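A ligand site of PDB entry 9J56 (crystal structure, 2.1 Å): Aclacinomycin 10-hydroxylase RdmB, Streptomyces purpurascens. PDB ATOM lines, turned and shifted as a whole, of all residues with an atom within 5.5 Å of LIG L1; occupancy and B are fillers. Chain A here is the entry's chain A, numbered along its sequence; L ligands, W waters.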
ATOM      1  N   TRP A 109       0.693 -15.119  18.417  1.00  0.00           N
ATOM      2  CA  TRP A 109       0.969 -16.039  17.321  1.00  0.00           C
ATOM      3  C   TRP A 109       1.921 -17.155  17.756  1.00  0.00           C
ATOM      4  O   TRP A 109       1.783 -18.292  17.290  1.00  0.00           O
ATOM      5  CB  TRP A 109       1.521 -15.281  16.111  1.00  0.00           C
ATOM      6  CG  TRP A 109       0.434 -14.597  15.363  1.00  0.00           C
ATOM      7  CD1 TRP A 109      -0.258 -13.485  15.761  1.00  0.00           C
ATOM      8  CD2 TRP A 109      -0.138 -15.011  14.110  1.00  0.00           C
ATOM      9  NE1 TRP A 109      -1.221 -13.168  14.811  1.00  0.00           N
ATOM     10  CE2 TRP A 109      -1.162 -14.075  13.795  1.00  0.00           C
ATOM     11  CE3 TRP A 109       0.130 -16.041  13.214  1.00  0.00           C
ATOM     12  CZ2 TRP A 109      -1.915 -14.155  12.619  1.00  0.00           C
ATOM     13  CZ3 TRP A 109      -0.629 -16.136  12.044  1.00  0.00           C
ATOM     14  CH2 TRP A 109      -1.636 -15.190  11.767  1.00  0.00           C
ATOM     15  N   VAL A 116      -2.044 -21.476  15.845  1.00  0.00           N
ATOM     16  CA  VAL A 116      -1.017 -21.369  14.817  1.00  0.00           C
ATOM     17  C   VAL A 116       0.296 -21.968  15.303  1.00  0.00           C
ATOM     18  O   VAL A 116       0.945 -22.745  14.590  1.00  0.00           O
ATOM     19  CB  VAL A 116      -0.851 -19.901  14.369  1.00  0.00           C
ATOM     20  CG1 VAL A 116       0.479 -19.702  13.665  1.00  0.00           C
ATOM     21  CG2 VAL A 116      -1.983 -19.531  13.434  1.00  0.00           C
ATOM     22  N   PHE A 145      -6.527 -30.479  10.228  1.00  0.00           N
ATOM     23  CA  PHE A 145      -6.579 -29.151  10.819  1.00  0.00           C
ATOM     24  C   PHE A 145      -8.005 -28.678  11.089  1.00  0.00           C
ATOM     25  O   PHE A 145      -8.372 -28.362  12.224  1.00  0.00           O
ATOM     26  CB  PHE A 145      -5.835 -28.147   9.929  1.00  0.00           C
ATOM     27  CG  PHE A 145      -5.807 -26.739  10.471  1.00  0.00           C
ATOM     28  CD1 PHE A 145      -4.842 -26.364  11.394  1.00  0.00           C
ATOM     29  CD2 PHE A 145      -6.723 -25.798  10.050  1.00  0.00           C
ATOM     30  CE1 PHE A 145      -4.811 -25.070  11.908  1.00  0.00           C
ATOM     31  CE2 PHE A 145      -6.706 -24.500  10.561  1.00  0.00           C
ATOM     32  CZ  PHE A 145      -5.745 -24.139  11.481  1.00  0.00           C
ATOM     33  N   TRP A 146      -8.845 -28.601  10.040  1.00  0.00           N
ATOM     34  CA  TRP A 146     -10.178 -28.051  10.231  1.00  0.00           C
ATOM     35  C   TRP A 146     -11.035 -28.959  11.117  1.00  0.00           C
ATOM     36  O   TRP A 146     -11.756 -28.476  11.995  1.00  0.00           O
ATOM     37  CB  TRP A 146     -10.853 -27.798   8.877  1.00  0.00           C
ATOM     38  CG  TRP A 146     -10.166 -26.676   8.126  1.00  0.00           C
ATOM     39  CD1 TRP A 146      -9.458 -26.773   6.971  1.00  0.00           C
ATOM     40  CD2 TRP A 146     -10.093 -25.300   8.529  1.00  0.00           C
ATOM     41  NE1 TRP A 146      -8.948 -25.547   6.618  1.00  0.00           N
ATOM     42  CE2 TRP A 146      -9.323 -24.625   7.552  1.00  0.00           C
ATOM     43  CE3 TRP A 146     -10.603 -24.570   9.606  1.00  0.00           C
ATOM     44  CZ2 TRP A 146      -9.052 -23.249   7.630  1.00  0.00           C
ATOM     45  CZ3 TRP A 146     -10.332 -23.218   9.691  1.00  0.00           C
ATOM     46  CH2 TRP A 146      -9.569 -22.570   8.708  1.00  0.00           C
ATOM     47  N   PHE A 159      -7.775 -19.402  17.113  1.00  0.00           N
ATOM     48  CA  PHE A 159      -7.513 -19.131  15.707  1.00  0.00           C
ATOM     49  C   PHE A 159      -8.354 -17.963  15.216  1.00  0.00           C
ATOM     50  O   PHE A 159      -7.827 -17.014  14.616  1.00  0.00           O
ATOM     51  CB  PHE A 159      -7.792 -20.370  14.853  1.00  0.00           C
ATOM     52  CG  PHE A 159      -7.620 -20.116  13.421  1.00  0.00           C
ATOM     53  CD1 PHE A 159      -6.356 -19.840  12.911  1.00  0.00           C
ATOM     54  CD2 PHE A 159      -8.700 -20.062  12.577  1.00  0.00           C
ATOM     55  CE1 PHE A 159      -6.187 -19.577  11.574  1.00  0.00           C
ATOM     56  CE2 PHE A 159      -8.547 -19.773  11.239  1.00  0.00           C
ATOM     57  CZ  PHE A 159      -7.275 -19.539  10.746  1.00  0.00           C
ATOM     58  N   LEU A 162      -6.912 -14.793  16.410  1.00  0.00           N
ATOM     59  CA  LEU A 162      -5.701 -14.374  15.721  1.00  0.00           C
ATOM     60  C   LEU A 162      -6.026 -13.679  14.403  1.00  0.00           C
ATOM     61  O   LEU A 162      -5.387 -12.691  14.037  1.00  0.00           O
ATOM     62  CB  LEU A 162      -4.780 -15.575  15.464  1.00  0.00           C
ATOM     63  CG  LEU A 162      -3.963 -16.103  16.656  1.00  0.00           C
ATOM     64  CD1 LEU A 162      -3.210 -17.399  16.277  1.00  0.00           C
ATOM     65  CD2 LEU A 162      -2.998 -15.058  17.181  1.00  0.00           C
ATOM     66  N   MET A 163      -7.017 -14.209  13.669  1.00  0.00           N
ATOM     67  CA  MET A 163      -7.410 -13.714  12.354  1.00  0.00           C
ATOM     68  C   MET A 163      -8.182 -12.393  12.439  1.00  0.00           C
ATOM     69  O   MET A 163      -8.157 -11.580  11.505  1.00  0.00           O
ATOM     70  CB  MET A 163      -8.283 -14.774  11.663  1.00  0.00           C
ATOM     71  CG  MET A 163      -7.570 -15.895  10.882  1.00  0.00           C
ATOM     72  SD  MET A 163      -6.087 -15.435   9.936  1.00  0.00           S
ATOM     73  CE  MET A 163      -4.847 -16.010  11.066  1.00  0.00           C
ATOM     74  N   SER A 164      -8.877 -12.161  13.546  1.00  0.00           N
ATOM     75  CA  SER A 164      -9.831 -11.071  13.703  1.00  0.00           C
ATOM     76  C   SER A 164      -9.304  -9.898  14.508  1.00  0.00           C
ATOM     77  O   SER A 164     -10.057  -8.947  14.760  1.00  0.00           O
ATOM     78  CB  SER A 164     -11.099 -11.603  14.360  1.00  0.00           C
ATOM     79  OG  SER A 164     -10.879 -11.817  15.746  1.00  0.00           O
ATOM     80  N   ASP A 168      -4.215  -4.715  13.536  1.00  0.00           N
ATOM     81  CA  ASP A 168      -3.808  -4.603  12.144  1.00  0.00           C
ATOM     82  C   ASP A 168      -5.009  -4.100  11.358  1.00  0.00           C
ATOM     83  O   ASP A 168      -6.083  -4.703  11.417  1.00  0.00           O
ATOM     84  CB  ASP A 168      -3.331  -5.964  11.629  1.00  0.00           C
ATOM     85  CG  ASP A 168      -2.650  -5.903  10.260  1.00  0.00           C
ATOM     86  OD1 ASP A 168      -2.855  -4.934   9.488  1.00  0.00           O
ATOM     87  OD2 ASP A 168      -1.912  -6.862   9.961  1.00  0.00           O
ATOM     88  N   ALA A 170      -5.377  -4.044   8.171  1.00  0.00           N
ATOM     89  CA  ALA A 170      -5.568  -4.735   6.903  1.00  0.00           C
ATOM     90  C   ALA A 170      -7.048  -5.050   6.658  1.00  0.00           C
ATOM     91  O   ALA A 170      -7.507  -4.986   5.509  1.00  0.00           O
ATOM     92  CB  ALA A 170      -4.759  -6.035   6.883  1.00  0.00           C
ATOM     93  N   TYR A 171      -7.808  -5.363   7.704  1.00  0.00           N
ATOM     94  CA  TYR A 171      -9.216  -5.718   7.525  1.00  0.00           C
ATOM     95  C   TYR A 171     -10.034  -4.570   6.932  1.00  0.00           C
ATOM     96  O   TYR A 171     -11.096  -4.829   6.336  1.00  0.00           O
ATOM     97  CB  TYR A 171      -9.822  -6.174   8.841  1.00  0.00           C
ATOM     98  CG  TYR A 171     -10.074  -5.077   9.856  1.00  0.00           C
ATOM     99  CD1 TYR A 171      -9.062  -4.618  10.679  1.00  0.00           C
ATOM    100  CD2 TYR A 171     -11.343  -4.502   9.995  1.00  0.00           C
ATOM    101  CE1 TYR A 171      -9.291  -3.635  11.609  1.00  0.00           C
ATOM    102  CE2 TYR A 171     -11.574  -3.509  10.916  1.00  0.00           C
ATOM    103  CZ  TYR A 171     -10.553  -3.079  11.726  1.00  0.00           C
ATOM    104  OH  TYR A 171     -10.779  -2.094  12.647  1.00  0.00           O
ATOM    105  N   SER A 255     -11.731 -13.512   1.344  1.00  0.00           N
ATOM    106  CA  SER A 255     -10.548 -12.907   1.963  1.00  0.00           C
ATOM    107  C   SER A 255      -9.690 -14.009   2.605  1.00  0.00           C
ATOM    108  O   SER A 255     -10.087 -14.597   3.611  1.00  0.00           O
ATOM    109  CB  SER A 255     -10.967 -11.861   2.988  1.00  0.00           C
ATOM    110  OG  SER A 255      -9.831 -11.248   3.554  1.00  0.00           O
ATOM    111  N   PHE A 256      -8.502 -14.226   2.050  1.00  0.00           N
ATOM    112  CA  PHE A 256      -7.554 -15.218   2.567  1.00  0.00           C
ATOM    113  C   PHE A 256      -8.253 -16.529   2.876  1.00  0.00           C
ATOM    114  O   PHE A 256      -8.162 -17.092   3.964  1.00  0.00           O
ATOM    115  CB  PHE A 256      -6.790 -14.671   3.777  1.00  0.00           C
ATOM    116  CG  PHE A 256      -5.683 -13.737   3.370  1.00  0.00           C
ATOM    117  CD1 PHE A 256      -5.950 -12.391   3.112  1.00  0.00           C
ATOM    118  CD2 PHE A 256      -4.393 -14.219   3.157  1.00  0.00           C
ATOM    119  CE1 PHE A 256      -4.938 -11.534   2.688  1.00  0.00           C
ATOM    120  CE2 PHE A 256      -3.376 -13.372   2.733  1.00  0.00           C
ATOM    121  CZ  PHE A 256      -3.650 -12.030   2.504  1.00  0.00           C
ATOM    122  N   LEU A 259      -6.070 -19.749  -0.301  1.00  0.00           N
ATOM    123  CA  LEU A 259      -4.756 -20.289  -0.014  1.00  0.00           C
ATOM    124  C   LEU A 259      -4.798 -21.458   0.964  1.00  0.00           C
ATOM    125  O   LEU A 259      -3.771 -22.138   1.131  1.00  0.00           O
ATOM    126  CB  LEU A 259      -3.829 -19.196   0.540  1.00  0.00           C
ATOM    127  CG  LEU A 259      -3.959 -18.851   2.014  1.00  0.00           C
ATOM    128  CD1 LEU A 259      -2.671 -18.220   2.529  1.00  0.00           C
ATOM    129  CD2 LEU A 259      -5.151 -17.886   2.224  1.00  0.00           C
ATOM    130  N   ASN A 260      -5.935 -21.696   1.628  1.00  0.00           N
ATOM    131  CA  ASN A 260      -6.042 -22.832   2.531  1.00  0.00           C
ATOM    132  C   ASN A 260      -6.313 -24.124   1.807  1.00  0.00           C
ATOM    133  O   ASN A 260      -6.347 -25.183   2.449  1.00  0.00           O
ATOM    134  CB  ASN A 260      -7.174 -22.642   3.547  1.00  0.00           C
ATOM    135  CG  ASN A 260      -7.043 -21.407   4.382  1.00  0.00           C
ATOM    136  OD1 ASN A 260      -5.952 -20.853   4.592  1.00  0.00           O
ATOM    137  ND2 ASN A 260      -8.177 -20.975   4.912  1.00  0.00           N
ATOM    138  N   PHE A 300       8.313 -14.234   3.128  1.00  0.00           N
ATOM    139  CA  PHE A 300       7.011 -14.486   3.704  1.00  0.00           C
ATOM    140  C   PHE A 300       6.083 -15.220   2.746  1.00  0.00           C
ATOM    141  O   PHE A 300       5.181 -15.922   3.191  1.00  0.00           O
ATOM    142  CB  PHE A 300       6.403 -13.166   4.178  1.00  0.00           C
ATOM    143  CG  PHE A 300       7.178 -12.566   5.305  1.00  0.00           C
ATOM    144  CD1 PHE A 300       7.104 -13.120   6.570  1.00  0.00           C
ATOM    145  CD2 PHE A 300       8.034 -11.499   5.083  1.00  0.00           C
ATOM    146  CE1 PHE A 300       7.871 -12.605   7.619  1.00  0.00           C
ATOM    147  CE2 PHE A 300       8.799 -10.974   6.122  1.00  0.00           C
ATOM    148  CZ  PHE A 300       8.710 -11.526   7.393  1.00  0.00           C
ATOM    149  N   LEU A 303       7.338 -18.894   3.415  1.00  0.00           N
ATOM    150  CA  LEU A 303       6.989 -19.318   4.774  1.00  0.00           C
ATOM    151  C   LEU A 303       5.517 -19.653   4.873  1.00  0.00           C
ATOM    152  O   LEU A 303       5.144 -20.710   5.383  1.00  0.00           O
ATOM    153  CB  LEU A 303       7.374 -18.227   5.769  1.00  0.00           C
ATOM    154  CG  LEU A 303       6.926 -18.431   7.219  1.00  0.00           C
ATOM    155  CD1 LEU A 303       7.784 -19.475   7.871  1.00  0.00           C
ATOM    156  CD2 LEU A 303       7.009 -17.132   8.020  1.00  0.00           C
ATOM    157  N   LEU A 304       4.645 -18.733   4.429  1.00  0.00           N
ATOM    158  CA  LEU A 304       3.211 -18.989   4.468  1.00  0.00           C
ATOM    159  C   LEU A 304       2.829 -20.148   3.536  1.00  0.00           C
ATOM    160  O   LEU A 304       1.942 -20.933   3.867  1.00  0.00           O
ATOM    161  CB  LEU A 304       2.441 -17.711   4.107  1.00  0.00           C
ATOM    162  CG  LEU A 304       0.920 -17.763   3.997  1.00  0.00           C
ATOM    163  CD1 LEU A 304       0.249 -18.002   5.351  1.00  0.00           C
ATOM    164  CD2 LEU A 304       0.415 -16.470   3.342  1.00  0.00           C
ATOM    165  N   ARG A 307       3.558 -23.264   5.398  1.00  0.00           N
ATOM    166  CA  ARG A 307       2.568 -23.454   6.455  1.00  0.00           C
ATOM    167  C   ARG A 307       1.257 -23.971   5.889  1.00  0.00           C
ATOM    168  O   ARG A 307       0.667 -24.909   6.443  1.00  0.00           O
ATOM    169  CB  ARG A 307       2.351 -22.141   7.231  1.00  0.00           C
ATOM    170  CG  ARG A 307       3.370 -21.886   8.327  1.00  0.00           C
ATOM    171  CD  ARG A 307       3.038 -20.593   9.048  1.00  0.00           C
ATOM    172  NE  ARG A 307       3.743 -20.506  10.317  1.00  0.00           N
ATOM    173  CZ  ARG A 307       4.394 -19.433  10.763  1.00  0.00           C
ATOM    174  NH1 ARG A 307       4.440 -18.309  10.051  1.00  0.00           N
ATOM    175  NH2 ARG A 307       4.986 -19.479  11.950  1.00  0.00           N
ATOM    176  N   MET A 308       0.748 -23.371   4.800  1.00  0.00           N
ATOM    177  CA  MET A 308      -0.469 -23.902   4.194  1.00  0.00           C
ATOM    178  C   MET A 308      -0.296 -25.357   3.772  1.00  0.00           C
ATOM    179  O   MET A 308      -1.177 -26.196   4.002  1.00  0.00           O
ATOM    180  CB  MET A 308      -0.913 -23.057   3.004  1.00  0.00           C
ATOM    181  CG  MET A 308      -1.201 -21.553   3.299  1.00  0.00           C
ATOM    182  SD  MET A 308      -2.625 -21.542   4.408  1.00  0.00           S
ATOM    183  CE  MET A 308      -1.862 -21.297   6.000  1.00  0.00           C
ATOM    184  N   PHE A 311       0.130 -27.604   7.124  1.00  0.00           N
ATOM    185  CA  PHE A 311      -1.018 -27.608   8.021  1.00  0.00           C
ATOM    186  C   PHE A 311      -2.271 -28.229   7.391  1.00  0.00           C
ATOM    187  O   PHE A 311      -3.095 -28.807   8.096  1.00  0.00           O
ATOM    188  CB  PHE A 311      -1.403 -26.182   8.445  1.00  0.00           C
ATOM    189  CG  PHE A 311      -0.359 -25.474   9.252  1.00  0.00           C
ATOM    190  CD1 PHE A 311       0.769 -26.132   9.712  1.00  0.00           C
ATOM    191  CD2 PHE A 311      -0.534 -24.135   9.562  1.00  0.00           C
ATOM    192  CE1 PHE A 311       1.727 -25.449  10.461  1.00  0.00           C
ATOM    193  CE2 PHE A 311       0.411 -23.448  10.309  1.00  0.00           C
ATOM    194  CZ  PHE A 311       1.544 -24.104  10.749  1.00  0.00           C
ATOM    195  N   MET A 312      -2.489 -28.026   6.088  1.00  0.00           N
ATOM    196  CA  MET A 312      -3.766 -28.431   5.517  1.00  0.00           C
ATOM    197  C   MET A 312      -3.698 -28.743   4.031  1.00  0.00           C
ATOM    198  O   MET A 312      -4.758 -28.932   3.416  1.00  0.00           O
ATOM    199  CB  MET A 312      -4.872 -27.348   5.737  1.00  0.00           C
ATOM    200  CG  MET A 312      -4.541 -25.947   5.238  1.00  0.00           C
ATOM    201  SD  MET A 312      -5.580 -24.633   5.984  1.00  0.00           S
ATOM    202  CE  MET A 312      -4.557 -24.099   7.334  1.00  0.00           C
ATOM    203  N   SER A 341      -0.608  -5.395   5.399  1.00  0.00           N
ATOM    204  CA  SER A 341      -0.690  -5.264   6.842  1.00  0.00           C
ATOM    205  C   SER A 341      -0.059  -3.960   7.278  1.00  0.00           C
ATOM    206  O   SER A 341       0.917  -3.468   6.693  1.00  0.00           O
ATOM    207  CB  SER A 341       0.023  -6.448   7.517  1.00  0.00           C
ATOM    208  OG  SER A 341       0.230  -6.209   8.887  1.00  0.00           O
ATOM    209  N   LEU A 344       2.618  -5.944  10.286  1.00  0.00           N
ATOM    210  CA  LEU A 344       3.600  -6.912   9.821  1.00  0.00           C
ATOM    211  C   LEU A 344       4.164  -6.492   8.477  1.00  0.00           C
ATOM    212  O   LEU A 344       3.568  -5.666   7.778  1.00  0.00           O
ATOM    213  CB  LEU A 344       2.965  -8.311   9.684  1.00  0.00           C
ATOM    214  CG  LEU A 344       2.213  -8.781  10.927  1.00  0.00           C
ATOM    215  CD1 LEU A 344       1.438 -10.076  10.675  1.00  0.00           C
ATOM    216  CD2 LEU A 344       3.172  -8.941  12.111  1.00  0.00           C
ATOM    217  N   PHE A 346       3.969  -7.420   5.329  1.00  0.00           N
ATOM    218  CA  PHE A 346       3.193  -8.379   4.543  1.00  0.00           C
ATOM    219  C   PHE A 346       2.231  -7.635   3.618  1.00  0.00           C
ATOM    220  O   PHE A 346       1.113  -7.319   4.018  1.00  0.00           O
ATOM    221  CB  PHE A 346       2.449  -9.349   5.449  1.00  0.00           C
ATOM    222  CG  PHE A 346       1.836 -10.503   4.718  1.00  0.00           C
ATOM    223  CD1 PHE A 346       2.580 -11.655   4.474  1.00  0.00           C
ATOM    224  CD2 PHE A 346       0.537 -10.437   4.235  1.00  0.00           C
ATOM    225  CE1 PHE A 346       2.021 -12.720   3.792  1.00  0.00           C
ATOM    226  CE2 PHE A 346      -0.022 -11.503   3.553  1.00  0.00           C
ATOM    227  CZ  PHE A 346       0.722 -12.643   3.322  1.00  0.00           C
HETATM  228  O1  LIG L   1      -0.097 -19.451   9.836  1.00  0.00           O
HETATM  229  C1  LIG L   1      -1.001 -19.010   9.297  1.00  0.00           C
HETATM  230  C2  LIG L   1      -0.980 -17.625   8.745  1.00  0.00           C
HETATM  231  C3  LIG L   1      -2.041 -17.111   8.125  1.00  0.00           C
HETATM  232  C4  LIG L   1      -2.033 -15.815   7.618  1.00  0.00           C
HETATM  233  O2  LIG L   1      -3.144 -15.295   6.995  1.00  0.00           O
HETATM  234  C5  LIG L   1      -0.904 -15.043   7.778  1.00  0.00           C
HETATM  235  C6  LIG L   1      -0.914 -13.630   7.201  1.00  0.00           C
HETATM  236  O3  LIG L   1      -1.839 -12.790   7.912  1.00  0.00           O
HETATM  237  C7  LIG L   1      -2.669 -12.064   7.083  1.00  0.00           C
HETATM  238  O4  LIG L   1      -2.924 -10.691   7.596  1.00  0.00           O
HETATM  239  C8  LIG L   1      -3.812 -10.673   8.744  1.00  0.00           C
HETATM  240  C9  LIG L   1      -4.184  -9.252   9.003  1.00  0.00           C
HETATM  241  C10 LIG L   1      -5.069 -11.576   8.644  1.00  0.00           C
HETATM  242  O5  LIG L   1      -6.354 -10.976   8.992  1.00  0.00           O
HETATM  243  C11 LIG L   1      -5.245 -12.270   7.338  1.00  0.00           C
HETATM  244  N1  LIG L   1      -6.102 -11.397   6.419  1.00  0.00           N
HETATM  245  C12 LIG L   1      -3.980 -12.743   6.742  1.00  0.00           C
HETATM  246  C13 LIG L   1       0.491 -13.091   7.094  1.00  0.00           C
HETATM  247  C14 LIG L   1       1.456 -13.442   8.196  1.00  0.00           C
HETATM  248  C15 LIG L   1       2.890 -13.092   7.838  1.00  0.00           C
HETATM  249  C16 LIG L   1       3.538 -14.251   7.096  1.00  0.00           C
HETATM  250  O6  LIG L   1       1.060 -12.751   9.319  1.00  0.00           O
HETATM  251  C17 LIG L   1       1.509 -14.911   8.640  1.00  0.00           C
HETATM  252  C18 LIG L   1       0.168 -15.596   8.395  1.00  0.00           C
HETATM  253  C19 LIG L   1       0.158 -16.882   8.893  1.00  0.00           C
HETATM  254  O7  LIG L   1       1.253 -17.399   9.522  1.00  0.00           O
HETATM  255  C20 LIG L   1      -3.279 -17.922   7.961  1.00  0.00           C
HETATM  256  C21 LIG L   1      -3.331 -19.336   8.511  1.00  0.00           C
HETATM  257  C22 LIG L   1      -4.458 -20.130   8.379  1.00  0.00           C
HETATM  258  O8  LIG L   1      -5.551 -19.635   7.747  1.00  0.00           O
HETATM  259  C23 LIG L   1      -6.702 -20.375   7.900  1.00  0.00           C
HETATM  260  C24 LIG L   1      -4.486 -21.404   8.874  1.00  0.00           C
HETATM  261  C25 LIG L   1      -3.373 -21.899   9.522  1.00  0.00           C
HETATM  262  C26 LIG L   1      -2.255 -21.122   9.638  1.00  0.00           C
HETATM  263  C27 LIG L   1      -2.254 -19.841   9.137  1.00  0.00           C
HETATM  264  O9  LIG L   1      -4.156 -17.419   7.419  1.00  0.00           O
HETATM  265  N1  LG2 L   2     -11.894 -13.922   5.611  1.00  0.00           N
HETATM  266  C1  LG2 L   2     -11.119 -14.095   6.827  1.00  0.00           C
HETATM  267  C2  LG2 L   2     -10.213 -15.316   6.678  1.00  0.00           C
HETATM  268  C3  LG2 L   2     -10.330 -16.125   7.933  1.00  0.00           C
HETATM  269  S1  LG2 L   2      -9.341 -17.609   7.598  1.00  0.00           S
HETATM  270  C4  LG2 L   2     -10.263 -12.869   7.163  1.00  0.00           C
HETATM  271  O1  LG2 L   2     -10.105 -12.519   8.359  1.00  0.00           O
HETATM  272  O2  LG2 L   2      -9.712 -12.217   6.229  1.00  0.00           O
HETATM  273  C5  LG2 L   2     -10.290 -18.792   6.574  1.00  0.00           C
HETATM  274  C6  LG2 L   2     -11.767 -18.947   7.046  1.00  0.00           C
HETATM  275  O3  LG2 L   2     -12.313 -19.971   6.395  1.00  0.00           O
HETATM  276  C7  LG2 L   2     -11.891 -19.255   8.566  1.00  0.00           C
HETATM  277  O4  LG2 L   2     -12.567 -18.273   9.231  1.00  0.00           O
HETATM  278  C8  LG2 L   2     -12.686 -20.574   8.546  1.00  0.00           C
HETATM  279  O5  LG2 L   2     -13.724 -20.618   9.602  1.00  0.00           O
HETATM  280  C9  LG2 L   2     -13.372 -20.487   7.184  1.00  0.00           C
HETATM  281  N2  LG2 L   2     -13.787 -21.783   6.703  1.00  0.00           N
HETATM  282  C10 LG2 L   2     -13.046 -22.891   6.633  1.00  0.00           C
HETATM  283  N3  LG2 L   2     -13.803 -23.852   6.102  1.00  0.00           N
HETATM  284  C11 LG2 L   2     -15.007 -23.352   5.839  1.00  0.00           C
HETATM  285  C12 LG2 L   2     -16.138 -23.927   5.301  1.00  0.00           C
HETATM  286  N4  LG2 L   2     -16.310 -25.291   4.854  1.00  0.00           N
HETATM  287  N5  LG2 L   2     -17.241 -23.198   5.132  1.00  0.00           N
HETATM  288  C13 LG2 L   2     -17.245 -21.900   5.501  1.00  0.00           C
HETATM  289  N6  LG2 L   2     -16.130 -21.334   6.033  1.00  0.00           N
HETATM  290  C14 LG2 L   2     -15.006 -22.063   6.209  1.00  0.00           C
HETATM  291  O   HOH W   1       3.266 -17.405   7.870  1.00  0.00           O
HETATM  292  O   HOH W   2      -6.345  -7.001  10.046  1.00  0.00           O
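The side-chain hydroxyl (OG) of Ser 341 is in hydrogen-bond range of the backbone NH (N) of Leu 344, 2.8 Å away.
The indole nitrogen of Trp 146 is in hydrogen-bond range of the side-chain sulfur of Met 312 (3.5 Å).
The side-chain amide oxygen (OD1) of Asn 260 lies close to the side-chain sulfur (SD) of Met 308 (3.4 Å).
The side-chain carboxylate of Asp 168 is in hydrogen-bond range of the backbone NH of Ala 170 (3.0 Å).
OG of Ser 341 is in hydrogen-bond range of OD2 of Asp 168, 2.5 Å away.
The backbone carbonyl oxygen (O) of Phe 346 lies within hydrogen-bond range of the backbone NH (N) of Ser 341, at 2.9 Å.
Merely in contact with LIG L1: Phe 159 (3.0 Å), Leu 344 (3.0 Å), Met 312 (3.1 Å), Trp 109 (3.3 Å), Asp 168 (3.4 Å), Phe 256 (3.5 Å), Phe 311 (3.5 Å), Met 308 (3.5 Å), Leu 304 (3.6 Å), Phe 346 (3.6 Å), Trp 146 (3.7 Å), Phe 300 (3.8 Å), Phe 145 (3.8 Å), Val 116 (3.9 Å) and Ala 170 (3.9 Å).
18 residues have an atom within 4 Å of LIG L1: Trp 109, Val 116, Phe 145, Trp 146, Phe 159, Met 163, Asp 168, Ala 170, Phe 256, Asn 260, Phe 300, Leu 304, Arg 307, Met 308, Phe 311, Met 312, Leu 344 and Phe 346.
Water W1 bridges an oxygen (O7) of LIG L1 (2.6 Å) and the guanidinium group of Arg 307 (2.6 Å).
O of Met 163 is in hydrogen-bond range of O5 of LIG L1, at 3.2 Å.
The guanidinium group (NH1) of Arg 307 lies within hydrogen-bond range of an oxygen (O7) of LIG L1, 3.4 Å away.
The side-chain amide oxygen (OD1) of Asn 260 lies close to an oxygen (O8) of LIG L1.
O of Ser 255 sits at hydrogen-bond distance from N1 of LG2 L2.
The side-chain hydroxyl (OG) of Ser 255 is in hydrogen-bond range of an oxygen (O2) of LG2 L2.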
